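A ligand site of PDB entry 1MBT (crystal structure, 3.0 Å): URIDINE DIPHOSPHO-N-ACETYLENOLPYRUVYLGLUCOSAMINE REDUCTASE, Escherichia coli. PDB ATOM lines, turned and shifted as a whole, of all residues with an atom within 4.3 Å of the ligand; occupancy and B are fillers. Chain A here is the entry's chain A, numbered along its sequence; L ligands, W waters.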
ATOM      1  N   THR A  10     -19.210  31.721   3.014  1.00  0.00           N
ATOM      2  CA  THR A  10     -19.177  33.189   2.888  1.00  0.00           C
ATOM      3  C   THR A  10     -20.068  33.696   1.767  1.00  0.00           C
ATOM      4  O   THR A  10     -20.428  34.864   1.669  1.00  0.00           O
ATOM      5  CB  THR A  10     -17.824  33.744   2.567  1.00  0.00           C
ATOM      6  OG1 THR A  10     -17.285  32.863   1.578  1.00  0.00           O
ATOM      7  CG2 THR A  10     -17.033  33.990   3.814  1.00  0.00           C
ATOM      8  N   LEU A  44     -16.249  16.527   5.218  1.00  0.00           N
ATOM      9  CA  LEU A  44     -15.607  17.699   4.621  1.00  0.00           C
ATOM     10  C   LEU A  44     -14.978  18.611   5.696  1.00  0.00           C
ATOM     11  O   LEU A  44     -15.708  19.165   6.523  1.00  0.00           O
ATOM     12  CB  LEU A  44     -16.644  18.476   3.810  1.00  0.00           C
ATOM     13  CG  LEU A  44     -16.252  19.768   3.105  1.00  0.00           C
ATOM     14  CD1 LEU A  44     -15.716  19.461   1.727  1.00  0.00           C
ATOM     15  CD2 LEU A  44     -17.457  20.669   3.029  1.00  0.00           C
ATOM     16  N   ILE A  45     -13.654  18.780   5.813  1.00  0.00           N
ATOM     17  CA  ILE A  45     -13.108  19.647   6.871  1.00  0.00           C
ATOM     18  C   ILE A  45     -13.263  21.126   6.473  1.00  0.00           C
ATOM     19  O   ILE A  45     -13.151  21.467   5.300  1.00  0.00           O
ATOM     20  CB  ILE A  45     -11.601  19.429   7.116  1.00  0.00           C
ATOM     21  CG1 ILE A  45     -11.178  17.955   7.120  1.00  0.00           C
ATOM     22  CG2 ILE A  45     -11.321  20.111   8.441  1.00  0.00           C
ATOM     23  CD1 ILE A  45     -11.438  17.113   8.371  1.00  0.00           C
ATOM     24  N   LEU A  46     -13.465  22.051   7.386  1.00  0.00           N
ATOM     25  CA  LEU A  46     -13.681  23.418   6.961  1.00  0.00           C
ATOM     26  C   LEU A  46     -13.225  24.423   8.007  1.00  0.00           C
ATOM     27  O   LEU A  46     -13.275  24.150   9.202  1.00  0.00           O
ATOM     28  CB  LEU A  46     -15.179  23.508   6.670  1.00  0.00           C
ATOM     29  CG  LEU A  46     -15.889  24.487   5.787  1.00  0.00           C
ATOM     30  CD1 LEU A  46     -16.028  23.925   4.367  1.00  0.00           C
ATOM     31  CD2 LEU A  46     -17.265  24.746   6.383  1.00  0.00           C
ATOM     32  N   GLY A  47     -12.706  25.571   7.611  1.00  0.00           N
ATOM     33  CA  GLY A  47     -12.444  26.652   8.588  1.00  0.00           C
ATOM     34  C   GLY A  47     -13.616  27.648   8.618  1.00  0.00           C
ATOM     35  O   GLY A  47     -14.613  27.465   9.296  1.00  0.00           O
ATOM     36  N   GLU A  48     -13.574  28.684   7.787  1.00  0.00           N
ATOM     37  CA  GLU A  48     -14.675  29.669   7.706  1.00  0.00           C
ATOM     38  C   GLU A  48     -15.620  29.657   6.490  1.00  0.00           C
ATOM     39  O   GLU A  48     -16.358  30.602   6.224  1.00  0.00           O
ATOM     40  CB  GLU A  48     -14.095  31.049   7.788  1.00  0.00           C
ATOM     41  CG  GLU A  48     -13.428  31.297   9.097  1.00  0.00           C
ATOM     42  CD  GLU A  48     -13.071  32.754   9.350  1.00  0.00           C
ATOM     43  OE1 GLU A  48     -13.095  33.605   8.440  1.00  0.00           O
ATOM     44  OE2 GLU A  48     -12.759  33.007  10.515  1.00  0.00           O
ATOM     45  N   GLY A  49     -15.577  28.635   5.643  1.00  0.00           N
ATOM     46  CA  GLY A  49     -16.327  28.622   4.393  1.00  0.00           C
ATOM     47  C   GLY A  49     -15.928  29.668   3.341  1.00  0.00           C
ATOM     48  O   GLY A  49     -16.438  29.648   2.233  1.00  0.00           O
ATOM     49  N   SER A  50     -14.970  30.561   3.569  1.00  0.00           N
ATOM     50  CA  SER A  50     -14.605  31.602   2.596  1.00  0.00           C
ATOM     51  C   SER A  50     -14.069  31.288   1.213  1.00  0.00           C
ATOM     52  O   SER A  50     -13.803  32.183   0.419  1.00  0.00           O
ATOM     53  CB  SER A  50     -13.620  32.579   3.219  1.00  0.00           C
ATOM     54  OG  SER A  50     -12.439  32.018   3.732  1.00  0.00           O
ATOM     55  N   ASN A  51     -14.004  30.004   0.899  1.00  0.00           N
ATOM     56  CA  ASN A  51     -13.536  29.570  -0.414  1.00  0.00           C
ATOM     57  C   ASN A  51     -14.278  28.368  -1.003  1.00  0.00           C
ATOM     58  O   ASN A  51     -13.781  27.590  -1.822  1.00  0.00           O
ATOM     59  CB  ASN A  51     -12.058  29.241  -0.356  1.00  0.00           C
ATOM     60  CG  ASN A  51     -11.442  29.385  -1.734  1.00  0.00           C
ATOM     61  OD1 ASN A  51     -11.356  30.448  -2.314  1.00  0.00           O
ATOM     62  ND2 ASN A  51     -11.037  28.333  -2.385  1.00  0.00           N
ATOM     63  N   VAL A  52     -15.505  28.180  -0.536  1.00  0.00           N
ATOM     64  CA  VAL A  52     -16.365  27.151  -1.099  1.00  0.00           C
ATOM     65  C   VAL A  52     -17.682  27.699  -1.616  1.00  0.00           C
ATOM     66  O   VAL A  52     -18.220  28.727  -1.175  1.00  0.00           O
ATOM     67  CB  VAL A  52     -16.758  26.006  -0.099  1.00  0.00           C
ATOM     68  CG1 VAL A  52     -15.596  25.018   0.032  1.00  0.00           C
ATOM     69  CG2 VAL A  52     -17.196  26.585   1.233  1.00  0.00           C
ATOM     70  N   ASN A  65     -13.146  23.053  11.871  1.00  0.00           N
ATOM     71  CA  ASN A  65     -11.873  22.891  12.541  1.00  0.00           C
ATOM     72  C   ASN A  65     -11.491  24.091  13.409  1.00  0.00           C
ATOM     73  O   ASN A  65     -10.957  25.089  12.962  1.00  0.00           O
ATOM     74  CB  ASN A  65     -10.832  22.611  11.455  1.00  0.00           C
ATOM     75  CG  ASN A  65      -9.460  22.218  11.940  1.00  0.00           C
ATOM     76  OD1 ASN A  65      -8.966  22.767  12.914  1.00  0.00           O
ATOM     77  ND2 ASN A  65      -8.733  21.276  11.379  1.00  0.00           N
ATOM     78  N   ALA A  85      -4.511  24.978  13.215  1.00  0.00           N
ATOM     79  CA  ALA A  85      -5.380  25.101  12.062  1.00  0.00           C
ATOM     80  C   ALA A  85      -6.705  25.888  12.227  1.00  0.00           C
ATOM     81  O   ALA A  85      -7.203  26.494  11.259  1.00  0.00           O
ATOM     82  CB  ALA A  85      -5.681  23.709  11.592  1.00  0.00           C
ATOM     83  N   ILE A 110      -7.221  38.711   4.687  1.00  0.00           N
ATOM     84  CA  ILE A 110      -7.663  37.513   3.978  1.00  0.00           C
ATOM     85  C   ILE A 110      -8.488  36.728   5.014  1.00  0.00           C
ATOM     86  O   ILE A 110      -8.137  36.652   6.222  1.00  0.00           O
ATOM     87  CB  ILE A 110      -6.435  36.690   3.476  1.00  0.00           C
ATOM     88  CG1 ILE A 110      -5.610  37.576   2.521  1.00  0.00           C
ATOM     89  CG2 ILE A 110      -6.889  35.403   2.806  1.00  0.00           C
ATOM     90  CD1 ILE A 110      -4.411  36.952   1.815  1.00  0.00           C
ATOM     91  N   PRO A 111      -9.697  36.272   4.701  1.00  0.00           N
ATOM     92  CA  PRO A 111     -10.414  35.423   5.611  1.00  0.00           C
ATOM     93  C   PRO A 111      -9.964  33.975   5.576  1.00  0.00           C
ATOM     94  O   PRO A 111      -9.099  33.520   4.820  1.00  0.00           O
ATOM     95  CB  PRO A 111     -11.852  35.561   5.249  1.00  0.00           C
ATOM     96  CG  PRO A 111     -11.958  36.493   4.096  1.00  0.00           C
ATOM     97  CD  PRO A 111     -10.567  36.932   3.744  1.00  0.00           C
ATOM     98  N   GLY A 112     -10.559  33.281   6.517  1.00  0.00           N
ATOM     99  CA  GLY A 112     -10.274  31.883   6.703  1.00  0.00           C
ATOM    100  C   GLY A 112      -9.373  31.612   7.887  1.00  0.00           C
ATOM    101  O   GLY A 112      -8.964  32.489   8.636  1.00  0.00           O
ATOM    102  N   CYS A 113      -9.098  30.331   7.980  1.00  0.00           N
ATOM    103  CA  CYS A 113      -8.343  29.810   9.098  1.00  0.00           C
ATOM    104  C   CYS A 113      -6.900  29.509   8.743  1.00  0.00           C
ATOM    105  O   CYS A 113      -6.656  29.189   7.567  1.00  0.00           O
ATOM    106  CB  CYS A 113      -9.010  28.555   9.606  1.00  0.00           C
ATOM    107  SG  CYS A 113     -10.563  28.961  10.428  1.00  0.00           S
ATOM    108  N   SER A 116      -6.159  26.511   6.355  1.00  0.00           N
ATOM    109  CA  SER A 116      -6.567  26.673   4.964  1.00  0.00           C
ATOM    110  C   SER A 116      -5.488  27.185   4.042  1.00  0.00           C
ATOM    111  O   SER A 116      -5.240  26.746   2.930  1.00  0.00           O
ATOM    112  CB  SER A 116      -7.694  27.632   4.905  1.00  0.00           C
ATOM    113  OG  SER A 116      -8.830  27.121   4.232  1.00  0.00           O
ATOM    114  N   SER A 117      -4.727  28.110   4.622  1.00  0.00           N
ATOM    115  CA  SER A 117      -3.702  28.820   3.893  1.00  0.00           C
ATOM    116  C   SER A 117      -2.630  27.971   3.220  1.00  0.00           C
ATOM    117  O   SER A 117      -2.307  28.304   2.089  1.00  0.00           O
ATOM    118  CB  SER A 117      -3.028  29.855   4.809  1.00  0.00           C
ATOM    119  OG  SER A 117      -2.225  29.337   5.848  1.00  0.00           O
ATOM    120  N   ILE A 119      -3.248  25.195   1.771  1.00  0.00           N
ATOM    121  CA  ILE A 119      -3.996  24.466   0.764  1.00  0.00           C
ATOM    122  C   ILE A 119      -4.134  25.242  -0.512  1.00  0.00           C
ATOM    123  O   ILE A 119      -3.775  24.736  -1.577  1.00  0.00           O
ATOM    124  CB  ILE A 119      -5.375  24.089   1.268  1.00  0.00           C
ATOM    125  CG1 ILE A 119      -5.194  23.230   2.500  1.00  0.00           C
ATOM    126  CG2 ILE A 119      -6.098  23.262   0.257  1.00  0.00           C
ATOM    127  CD1 ILE A 119      -6.296  22.288   3.010  1.00  0.00           C
ATOM    128  N   GLN A 120      -4.605  26.474  -0.414  1.00  0.00           N
ATOM    129  CA  GLN A 120      -4.687  27.285  -1.623  1.00  0.00           C
ATOM    130  C   GLN A 120      -3.464  28.198  -1.709  1.00  0.00           C
ATOM    131  O   GLN A 120      -3.311  28.861  -2.717  1.00  0.00           O
ATOM    132  CB  GLN A 120      -5.954  28.152  -1.662  1.00  0.00           C
ATOM    133  CG  GLN A 120      -7.088  28.036  -0.617  1.00  0.00           C
ATOM    134  CD  GLN A 120      -7.866  26.727  -0.607  1.00  0.00           C
ATOM    135  OE1 GLN A 120      -8.385  26.291   0.396  1.00  0.00           O
ATOM    136  NE2 GLN A 120      -8.013  25.942  -1.628  1.00  0.00           N
ATOM    137  N   ILE A 122      -2.431  31.085   0.027  1.00  0.00           N
ATOM    138  CA  ILE A 122      -3.026  32.414   0.001  1.00  0.00           C
ATOM    139  C   ILE A 122      -2.071  33.533  -0.449  1.00  0.00           C
ATOM    140  O   ILE A 122      -0.936  33.676   0.015  1.00  0.00           O
ATOM    141  CB  ILE A 122      -3.642  32.787   1.414  1.00  0.00           C
ATOM    142  CG1 ILE A 122      -2.645  32.588   2.541  1.00  0.00           C
ATOM    143  CG2 ILE A 122      -4.882  31.932   1.660  1.00  0.00           C
ATOM    144  CD1 ILE A 122      -3.065  33.395   3.775  1.00  0.00           C
ATOM    145  N   GLY A 123      -2.532  34.245  -1.467  1.00  0.00           N
ATOM    146  CA  GLY A 123      -1.767  35.317  -2.056  1.00  0.00           C
ATOM    147  C   GLY A 123      -2.499  36.641  -2.062  1.00  0.00           C
ATOM    148  O   GLY A 123      -3.729  36.711  -1.989  1.00  0.00           O
ATOM    149  N   ALA A 124      -1.667  37.668  -1.976  1.00  0.00           N
ATOM    150  CA  ALA A 124      -2.082  39.059  -2.037  1.00  0.00           C
ATOM    151  C   ALA A 124      -0.895  39.997  -2.084  1.00  0.00           C
ATOM    152  O   ALA A 124       0.147  39.726  -1.464  1.00  0.00           O
ATOM    153  CB  ALA A 124      -2.888  39.475  -0.821  1.00  0.00           C
ATOM    154  N   ARG A 159      -1.565  29.477  -6.478  1.00  0.00           N
ATOM    155  CA  ARG A 159      -2.852  28.922  -6.061  1.00  0.00           C
ATOM    156  C   ARG A 159      -2.904  27.399  -5.960  1.00  0.00           C
ATOM    157  O   ARG A 159      -3.935  26.732  -6.082  1.00  0.00           O
ATOM    158  CB  ARG A 159      -3.917  29.436  -7.019  1.00  0.00           C
ATOM    159  CG  ARG A 159      -4.789  30.442  -6.293  1.00  0.00           C
ATOM    160  CD  ARG A 159      -3.924  31.578  -5.846  1.00  0.00           C
ATOM    161  NE  ARG A 159      -4.659  32.581  -5.146  1.00  0.00           N
ATOM    162  CZ  ARG A 159      -3.995  33.616  -4.642  1.00  0.00           C
ATOM    163  NH1 ARG A 159      -2.669  33.733  -4.762  1.00  0.00           N
ATOM    164  NH2 ARG A 159      -4.652  34.545  -3.966  1.00  0.00           N
ATOM    165  N   PHE A 171      -5.681  13.619   4.128  1.00  0.00           N
ATOM    166  CA  PHE A 171      -5.060  14.433   5.150  1.00  0.00           C
ATOM    167  C   PHE A 171      -5.896  15.580   5.675  1.00  0.00           C
ATOM    168  O   PHE A 171      -6.721  16.151   4.976  1.00  0.00           O
ATOM    169  CB  PHE A 171      -3.758  15.015   4.658  1.00  0.00           C
ATOM    170  CG  PHE A 171      -2.704  13.946   4.673  1.00  0.00           C
ATOM    171  CD1 PHE A 171      -2.556  13.086   3.589  1.00  0.00           C
ATOM    172  CD2 PHE A 171      -1.883  13.824   5.794  1.00  0.00           C
ATOM    173  CE1 PHE A 171      -1.587  12.096   3.621  1.00  0.00           C
ATOM    174  CE2 PHE A 171      -0.913  12.834   5.809  1.00  0.00           C
ATOM    175  CZ  PHE A 171      -0.765  11.974   4.725  1.00  0.00           C
ATOM    176  N   ALA A 172      -5.678  15.880   6.956  1.00  0.00           N
ATOM    177  CA  ALA A 172      -6.346  17.003   7.602  1.00  0.00           C
ATOM    178  C   ALA A 172      -5.348  17.887   8.301  1.00  0.00           C
ATOM    179  O   ALA A 172      -4.600  17.427   9.181  1.00  0.00           O
ATOM    180  CB  ALA A 172      -7.340  16.571   8.680  1.00  0.00           C
ATOM    181  N   ILE A 173      -5.307  19.159   7.915  1.00  0.00           N
ATOM    182  CA  ILE A 173      -4.335  20.022   8.543  1.00  0.00           C
ATOM    183  C   ILE A 173      -4.673  20.454   9.950  1.00  0.00           C
ATOM    184  O   ILE A 173      -5.787  20.850  10.245  1.00  0.00           O
ATOM    185  CB  ILE A 173      -4.144  21.166   7.582  1.00  0.00           C
ATOM    186  CG1 ILE A 173      -3.613  20.650   6.256  1.00  0.00           C
ATOM    187  CG2 ILE A 173      -3.168  22.176   8.192  1.00  0.00           C
ATOM    188  CD1 ILE A 173      -3.513  21.775   5.227  1.00  0.00           C
ATOM    189  N   ARG A 214      -8.029  46.923   0.341  1.00  0.00           N
ATOM    190  CA  ARG A 214      -9.021  45.863   0.471  1.00  0.00           C
ATOM    191  C   ARG A 214     -10.408  46.314   0.904  1.00  0.00           C
ATOM    192  O   ARG A 214     -11.411  46.038   0.251  1.00  0.00           O
ATOM    193  CB  ARG A 214      -8.487  44.826   1.453  1.00  0.00           C
ATOM    194  CG  ARG A 214      -7.274  44.134   0.858  1.00  0.00           C
ATOM    195  CD  ARG A 214      -6.887  42.929   1.693  1.00  0.00           C
ATOM    196  NE  ARG A 214      -6.923  41.727   0.881  1.00  0.00           N
ATOM    197  CZ  ARG A 214      -7.980  40.922   0.919  1.00  0.00           C
ATOM    198  NH1 ARG A 214      -9.032  41.197   1.704  1.00  0.00           N
ATOM    199  NH2 ARG A 214      -8.006  39.871   0.102  1.00  0.00           N
ATOM    200  N   LEU A 218     -12.872  45.704  -2.304  1.00  0.00           N
ATOM    201  CA  LEU A 218     -13.573  44.423  -2.220  1.00  0.00           C
ATOM    202  C   LEU A 218     -14.928  44.449  -1.490  1.00  0.00           C
ATOM    203  O   LEU A 218     -15.159  45.238  -0.573  1.00  0.00           O
ATOM    204  CB  LEU A 218     -12.672  43.375  -1.550  1.00  0.00           C
ATOM    205  CG  LEU A 218     -11.406  42.895  -2.258  1.00  0.00           C
ATOM    206  CD1 LEU A 218     -10.703  41.946  -1.328  1.00  0.00           C
ATOM    207  CD2 LEU A 218     -11.704  42.145  -3.537  1.00  0.00           C
ATOM    208  N   PRO A 219     -15.908  43.635  -1.892  1.00  0.00           N
ATOM    209  CA  PRO A 219     -17.172  43.462  -1.167  1.00  0.00           C
ATOM    210  C   PRO A 219     -17.183  42.722   0.175  1.00  0.00           C
ATOM    211  O   PRO A 219     -16.878  41.516   0.281  1.00  0.00           O
ATOM    212  CB  PRO A 219     -18.108  42.744  -2.105  1.00  0.00           C
ATOM    213  CG  PRO A 219     -17.322  42.442  -3.357  1.00  0.00           C
ATOM    214  CD  PRO A 219     -15.926  43.013  -3.206  1.00  0.00           C
ATOM    215  N   ASN A 226     -19.823  36.567  -0.902  1.00  0.00           N
ATOM    216  CA  ASN A 226     -18.842  36.170  -1.905  1.00  0.00           C
ATOM    217  C   ASN A 226     -17.729  35.256  -1.425  1.00  0.00           C
ATOM    218  O   ASN A 226     -17.573  34.963  -0.240  1.00  0.00           O
ATOM    219  CB  ASN A 226     -18.193  37.383  -2.542  1.00  0.00           C
ATOM    220  CG  ASN A 226     -17.387  38.221  -1.589  1.00  0.00           C
ATOM    221  OD1 ASN A 226     -16.194  38.093  -1.526  1.00  0.00           O
ATOM    222  ND2 ASN A 226     -17.866  39.055  -0.729  1.00  0.00           N
ATOM    223  N   ALA A 227     -16.960  34.739  -2.360  1.00  0.00           N
ATOM    224  CA  ALA A 227     -15.778  33.973  -2.008  1.00  0.00           C
ATOM    225  C   ALA A 227     -14.564  34.779  -2.510  1.00  0.00           C
ATOM    226  O   ALA A 227     -13.587  34.286  -3.068  1.00  0.00           O
ATOM    227  CB  ALA A 227     -15.890  32.626  -2.679  1.00  0.00           C
ATOM    228  N   GLY A 228     -14.603  36.102  -2.322  1.00  0.00           N
ATOM    229  CA  GLY A 228     -13.652  37.037  -2.928  1.00  0.00           C
ATOM    230  C   GLY A 228     -13.505  36.920  -4.464  1.00  0.00           C
ATOM    231  O   GLY A 228     -14.446  36.806  -5.246  1.00  0.00           O
ATOM    232  N   GLU A 325     -11.019  29.943  -8.604  1.00  0.00           N
ATOM    233  CA  GLU A 325     -10.215  29.699  -7.431  1.00  0.00           C
ATOM    234  C   GLU A 325     -11.087  29.019  -6.363  1.00  0.00           C
ATOM    235  O   GLU A 325     -10.615  28.228  -5.546  1.00  0.00           O
ATOM    236  CB  GLU A 325      -9.670  31.014  -6.894  1.00  0.00           C
ATOM    237  CG  GLU A 325      -8.691  30.792  -5.751  1.00  0.00           C
ATOM    238  CD  GLU A 325      -8.181  32.036  -5.025  1.00  0.00           C
ATOM    239  OE1 GLU A 325      -8.453  33.171  -5.430  1.00  0.00           O
ATOM    240  OE2 GLU A 325      -7.486  31.856  -4.033  1.00  0.00           O
ATOM    241  N   ARG A 327     -13.751  26.589  -4.470  1.00  0.00           N
ATOM    242  CA  ARG A 327     -13.919  25.150  -4.526  1.00  0.00           C
ATOM    243  C   ARG A 327     -15.367  24.698  -4.547  1.00  0.00           C
ATOM    244  O   ARG A 327     -16.220  25.045  -3.727  1.00  0.00           O
ATOM    245  CB  ARG A 327     -13.148  24.561  -3.332  1.00  0.00           C
ATOM    246  CG  ARG A 327     -11.693  24.969  -3.611  1.00  0.00           C
ATOM    247  CD  ARG A 327     -10.555  24.484  -2.753  1.00  0.00           C
ATOM    248  NE  ARG A 327     -10.231  23.105  -3.027  1.00  0.00           N
ATOM    249  CZ  ARG A 327      -9.322  22.479  -2.293  1.00  0.00           C
ATOM    250  NH1 ARG A 327      -8.664  23.092  -1.321  1.00  0.00           N
ATOM    251  NH2 ARG A 327      -9.171  21.169  -2.422  1.00  0.00           N
ATOM    252  N   GLU A 334     -16.214  17.010  -3.556  1.00  0.00           N
ATOM    253  CA  GLU A 334     -15.745  18.044  -4.493  1.00  0.00           C
ATOM    254  C   GLU A 334     -15.817  17.671  -5.961  1.00  0.00           C
ATOM    255  O   GLU A 334     -15.596  16.523  -6.340  1.00  0.00           O
ATOM    256  CB  GLU A 334     -14.276  18.429  -4.141  1.00  0.00           C
ATOM    257  CG  GLU A 334     -13.636  19.610  -4.905  1.00  0.00           C
ATOM    258  CD  GLU A 334     -12.374  20.251  -4.306  1.00  0.00           C
ATOM    259  OE1 GLU A 334     -12.072  20.045  -3.136  1.00  0.00           O
ATOM    260  OE2 GLU A 334     -11.690  20.984  -5.015  1.00  0.00           O
HETATM  261  P1  LIG L   1     -12.570  26.976   3.558  1.00  0.00           P
HETATM  262  O1  LIG L   1     -13.317  26.694   4.848  1.00  0.00           O
HETATM  263  O2  LIG L   1     -13.422  27.585   2.463  1.00  0.00           O
HETATM  264  O3  LIG L   1     -11.862  25.641   3.031  1.00  0.00           O
HETATM  265  C1  LIG L   1     -11.191  25.705   1.777  1.00  0.00           C
HETATM  266  C2  LIG L   1     -10.775  24.330   1.283  1.00  0.00           C
HETATM  267  O4  LIG L   1      -9.740  23.832   2.169  1.00  0.00           O
HETATM  268  C3  LIG L   1     -11.827  23.258   1.315  1.00  0.00           C
HETATM  269  O5  LIG L   1     -11.535  22.336   0.218  1.00  0.00           O
HETATM  270  C4  LIG L   1     -11.672  22.631   2.708  1.00  0.00           C
HETATM  271  O6  LIG L   1     -12.126  21.280   2.830  1.00  0.00           O
HETATM  272  C5  LIG L   1     -10.186  22.719   2.940  1.00  0.00           C
HETATM  273  N1  LIG L   1      -9.729  22.962   4.276  1.00  0.00           N
HETATM  274  C6  LIG L   1     -10.150  24.099   4.879  1.00  0.00           C
HETATM  275  N2  LIG L   1      -9.571  23.962   6.200  1.00  0.00           N
HETATM  276  C7  LIG L   1      -8.914  22.613   6.230  1.00  0.00           C
HETATM  277  C8  LIG L   1      -8.175  21.726   7.156  1.00  0.00           C
HETATM  278  N3  LIG L   1      -7.889  22.100   8.394  1.00  0.00           N
HETATM  279  N4  LIG L   1      -7.777  20.484   6.736  1.00  0.00           N
HETATM  280  C9  LIG L   1      -8.084  20.100   5.479  1.00  0.00           C
HETATM  281  N5  LIG L   1      -8.705  20.785   4.566  1.00  0.00           N
HETATM  282  C10 LIG L   1      -9.090  22.042   5.033  1.00  0.00           C
HETATM  283  N6  LIG L   1      -7.956  33.771  -1.003  1.00  0.00           N
HETATM  284  C11 LIG L   1      -6.657  34.016  -1.384  1.00  0.00           C
HETATM  285  O7  LIG L   1      -5.906  33.123  -1.673  1.00  0.00           O
HETATM  286  N7  LIG L   1      -6.222  35.298  -1.427  1.00  0.00           N
HETATM  287  C12 LIG L   1      -6.963  36.358  -1.098  1.00  0.00           C
HETATM  288  O8  LIG L   1      -6.541  37.489  -1.101  1.00  0.00           O
HETATM  289  C13 LIG L   1      -8.424  36.135  -0.715  1.00  0.00           C
HETATM  290  N8  LIG L   1      -9.281  37.176  -0.399  1.00  0.00           N
HETATM  291  C14 LIG L   1     -10.597  36.937  -0.093  1.00  0.00           C
HETATM  292  C15 LIG L   1     -11.474  37.997   0.129  1.00  0.00           C
HETATM  293  C16 LIG L   1     -12.808  37.752   0.497  1.00  0.00           C
HETATM  294  C17 LIG L   1     -13.750  38.914   0.686  1.00  0.00           C
HETATM  295  C18 LIG L   1     -13.235  36.423   0.673  1.00  0.00           C
HETATM  296  C19 LIG L   1     -14.667  36.307   1.127  1.00  0.00           C
HETATM  297  C20 LIG L   1     -12.338  35.394   0.423  1.00  0.00           C
HETATM  298  C21 LIG L   1     -11.008  35.636   0.009  1.00  0.00           C
HETATM  299  N9  LIG L   1     -10.120  34.571  -0.294  1.00  0.00           N
HETATM  300  C22 LIG L   1      -8.820  34.754  -0.676  1.00  0.00           C
HETATM  301  C23 LIG L   1     -10.520  33.149  -0.249  1.00  0.00           C
HETATM  302  C24 LIG L   1     -10.284  32.550   1.148  1.00  0.00           C
HETATM  303  O9  LIG L   1     -10.175  33.513   2.185  1.00  0.00           O
HETATM  304  C25 LIG L   1      -9.039  31.640   1.128  1.00  0.00           C
HETATM  305  O10 LIG L   1      -9.043  30.752   0.029  1.00  0.00           O
HETATM  306  C26 LIG L   1      -8.873  30.893   2.464  1.00  0.00           C
HETATM  307  O11 LIG L   1      -7.730  30.048   2.484  1.00  0.00           O
HETATM  308  C27 LIG L   1     -10.128  30.113   2.866  1.00  0.00           C
HETATM  309  O12 LIG L   1     -10.333  30.279   4.270  1.00  0.00           O
HETATM  310  P2  LIG L   1     -11.184  29.163   4.894  1.00  0.00           P
HETATM  311  O13 LIG L   1     -10.453  28.690   6.137  1.00  0.00           O
HETATM  312  O14 LIG L   1     -12.532  29.767   5.197  1.00  0.00           O
HETATM  313  O15 LIG L   1     -11.361  27.909   3.842  1.00  0.00           O
HETATM  314  O   HOH W   1      -6.885  31.780   5.006  1.00  0.00           O
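Water W1 bridges O of Pro 111 and O11 of the ligand.
O7 of the ligand lies close to OE2 of Glu 325, 3.1 Å away.
Merely in contact with the ligand: Gly 112 (2.9 Å), Ile 119 (3.2 Å), Gly 228 (3.3 Å), Asn 226 (3.4 Å), Ile 122 (3.4 Å), Leu 46 (3.5 Å), Ile 110 (3.7 Å), Val 52 (3.7 Å), Ala 227 (3.7 Å) and Ala 172 (3.9 Å).
27 residues have an atom within 4 Å of the ligand: Ile 45, Leu 46, Gly 47, Glu 48, Gly 49, Ser 50, Asn 51, Val 52, Asn 65, Ile 110, Pro 111, Gly 112, Cys 113, Ser 116, Ile 119, Gln 120, Ile 122, Gly 123, Arg 159, Ala 172, Ile 173, Arg 214, Asn 226, Ala 227, Gly 228, Glu 325 and Arg 327.
Along chain A the residues within 4 Å of the ligand span positions 45 to 327.
The nearest printed residue that does not touch the ligand is Pro 219 (4.1 Å).
The side-chain hydroxyl (OG) of Ser 116 lies within hydrogen-bond range of an oxygen (O15) of the ligand, 2.7 Å away.
O of Ile 45 lies within hydrogen-bond range of O6 of the ligand (2.7 Å).
An oxygen (O14) of the ligand lies within hydrogen-bond range of the backbone NH (N) of Ser 50 (3.0 Å).
OG of Ser 50 is in hydrogen-bond range of O14 of the ligand, 2.7 Å away.
The backbone NH of Cys 113 lies within hydrogen-bond range of an oxygen (O13) of the ligand, 2.8 Å away.
The backbone carbonyl oxygen (O) of Pro 111 lies within hydrogen-bond range of an oxygen (O9) of the ligand, 2.8 Å away.
O of Gly 123 sits at hydrogen-bond distance from N7 of the ligand.
The backbone NH (N) of Asn 51 lies within hydrogen-bond range of an oxygen (O2) of the ligand, at 2.9 Å.
OD1 of Asn 51 lies close to O10 of the ligand (3.3 Å).
NH2 of Arg 159 is in hydrogen-bond range of O7 of the ligand.
An oxygen (O14) of the ligand sits at hydrogen-bond distance from the backbone NH (N) of Glu 48 (3.0 Å).
N8 of the ligand is in hydrogen-bond range of NH2 of Arg 214 (3.0 Å).
A nitrogen (N4) of the ligand lies within hydrogen-bond range of the backbone NH of Ile 173, 3.0 Å away.
A nitrogen (N3) of the ligand is in hydrogen-bond range of the backbone carbonyl oxygen (O) of Ile 173, at 3.1 Å.
The backbone NH (N) of Gly 47 sits at hydrogen-bond distance from an oxygen (O1) of the ligand (3.0 Å).
N of Gly 49 is in hydrogen-bond range of O1 of the ligand (3.1 Å).
The side-chain amide oxygen of Gln 120 lies close to an oxygen (O4) of the ligand, 3.3 Å away.
The side-chain amide nitrogen (ND2) of Asn 65 sits close to a nitrogen (N3) of the ligand, at 3.2 Å.
NH1 of Arg 327 lies within hydrogen-bond range of O5 of the ligand (3.3 Å).
The backbone NH of Gly 112 is in hydrogen-bond range of the side-chain carboxylate of Glu 48.
ND2 of Asn 51 sits at hydrogen-bond distance from O of Glu 325 (3.2 Å).
The backbone carbonyl oxygen of Ile 173 sits at hydrogen-bond distance from the side-chain amide nitrogen of Asn 65, 3.2 Å away.
The backbone carbonyl oxygen (O) of Gly 49 sits at hydrogen-bond distance from the side-chain hydroxyl (OG1) of Thr 10 (3.4 Å).
The side-chain amide nitrogen (NE2) of Gln 120 sits close to the guanidinium group (NH1) of Arg 327, 2.9 Å away.
NH2 of Arg 327 is in salt-bridge range of OE1 of Glu 334, 3.2 Å away.
The backbone carbonyl oxygen (O) of Pro 219 lies within hydrogen-bond range of the side-chain amide nitrogen (ND2) of Asn 226 (2.8 Å).
O of Asn 226 is in hydrogen-bond range of OG1 of Thr 10, 2.8 Å away.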
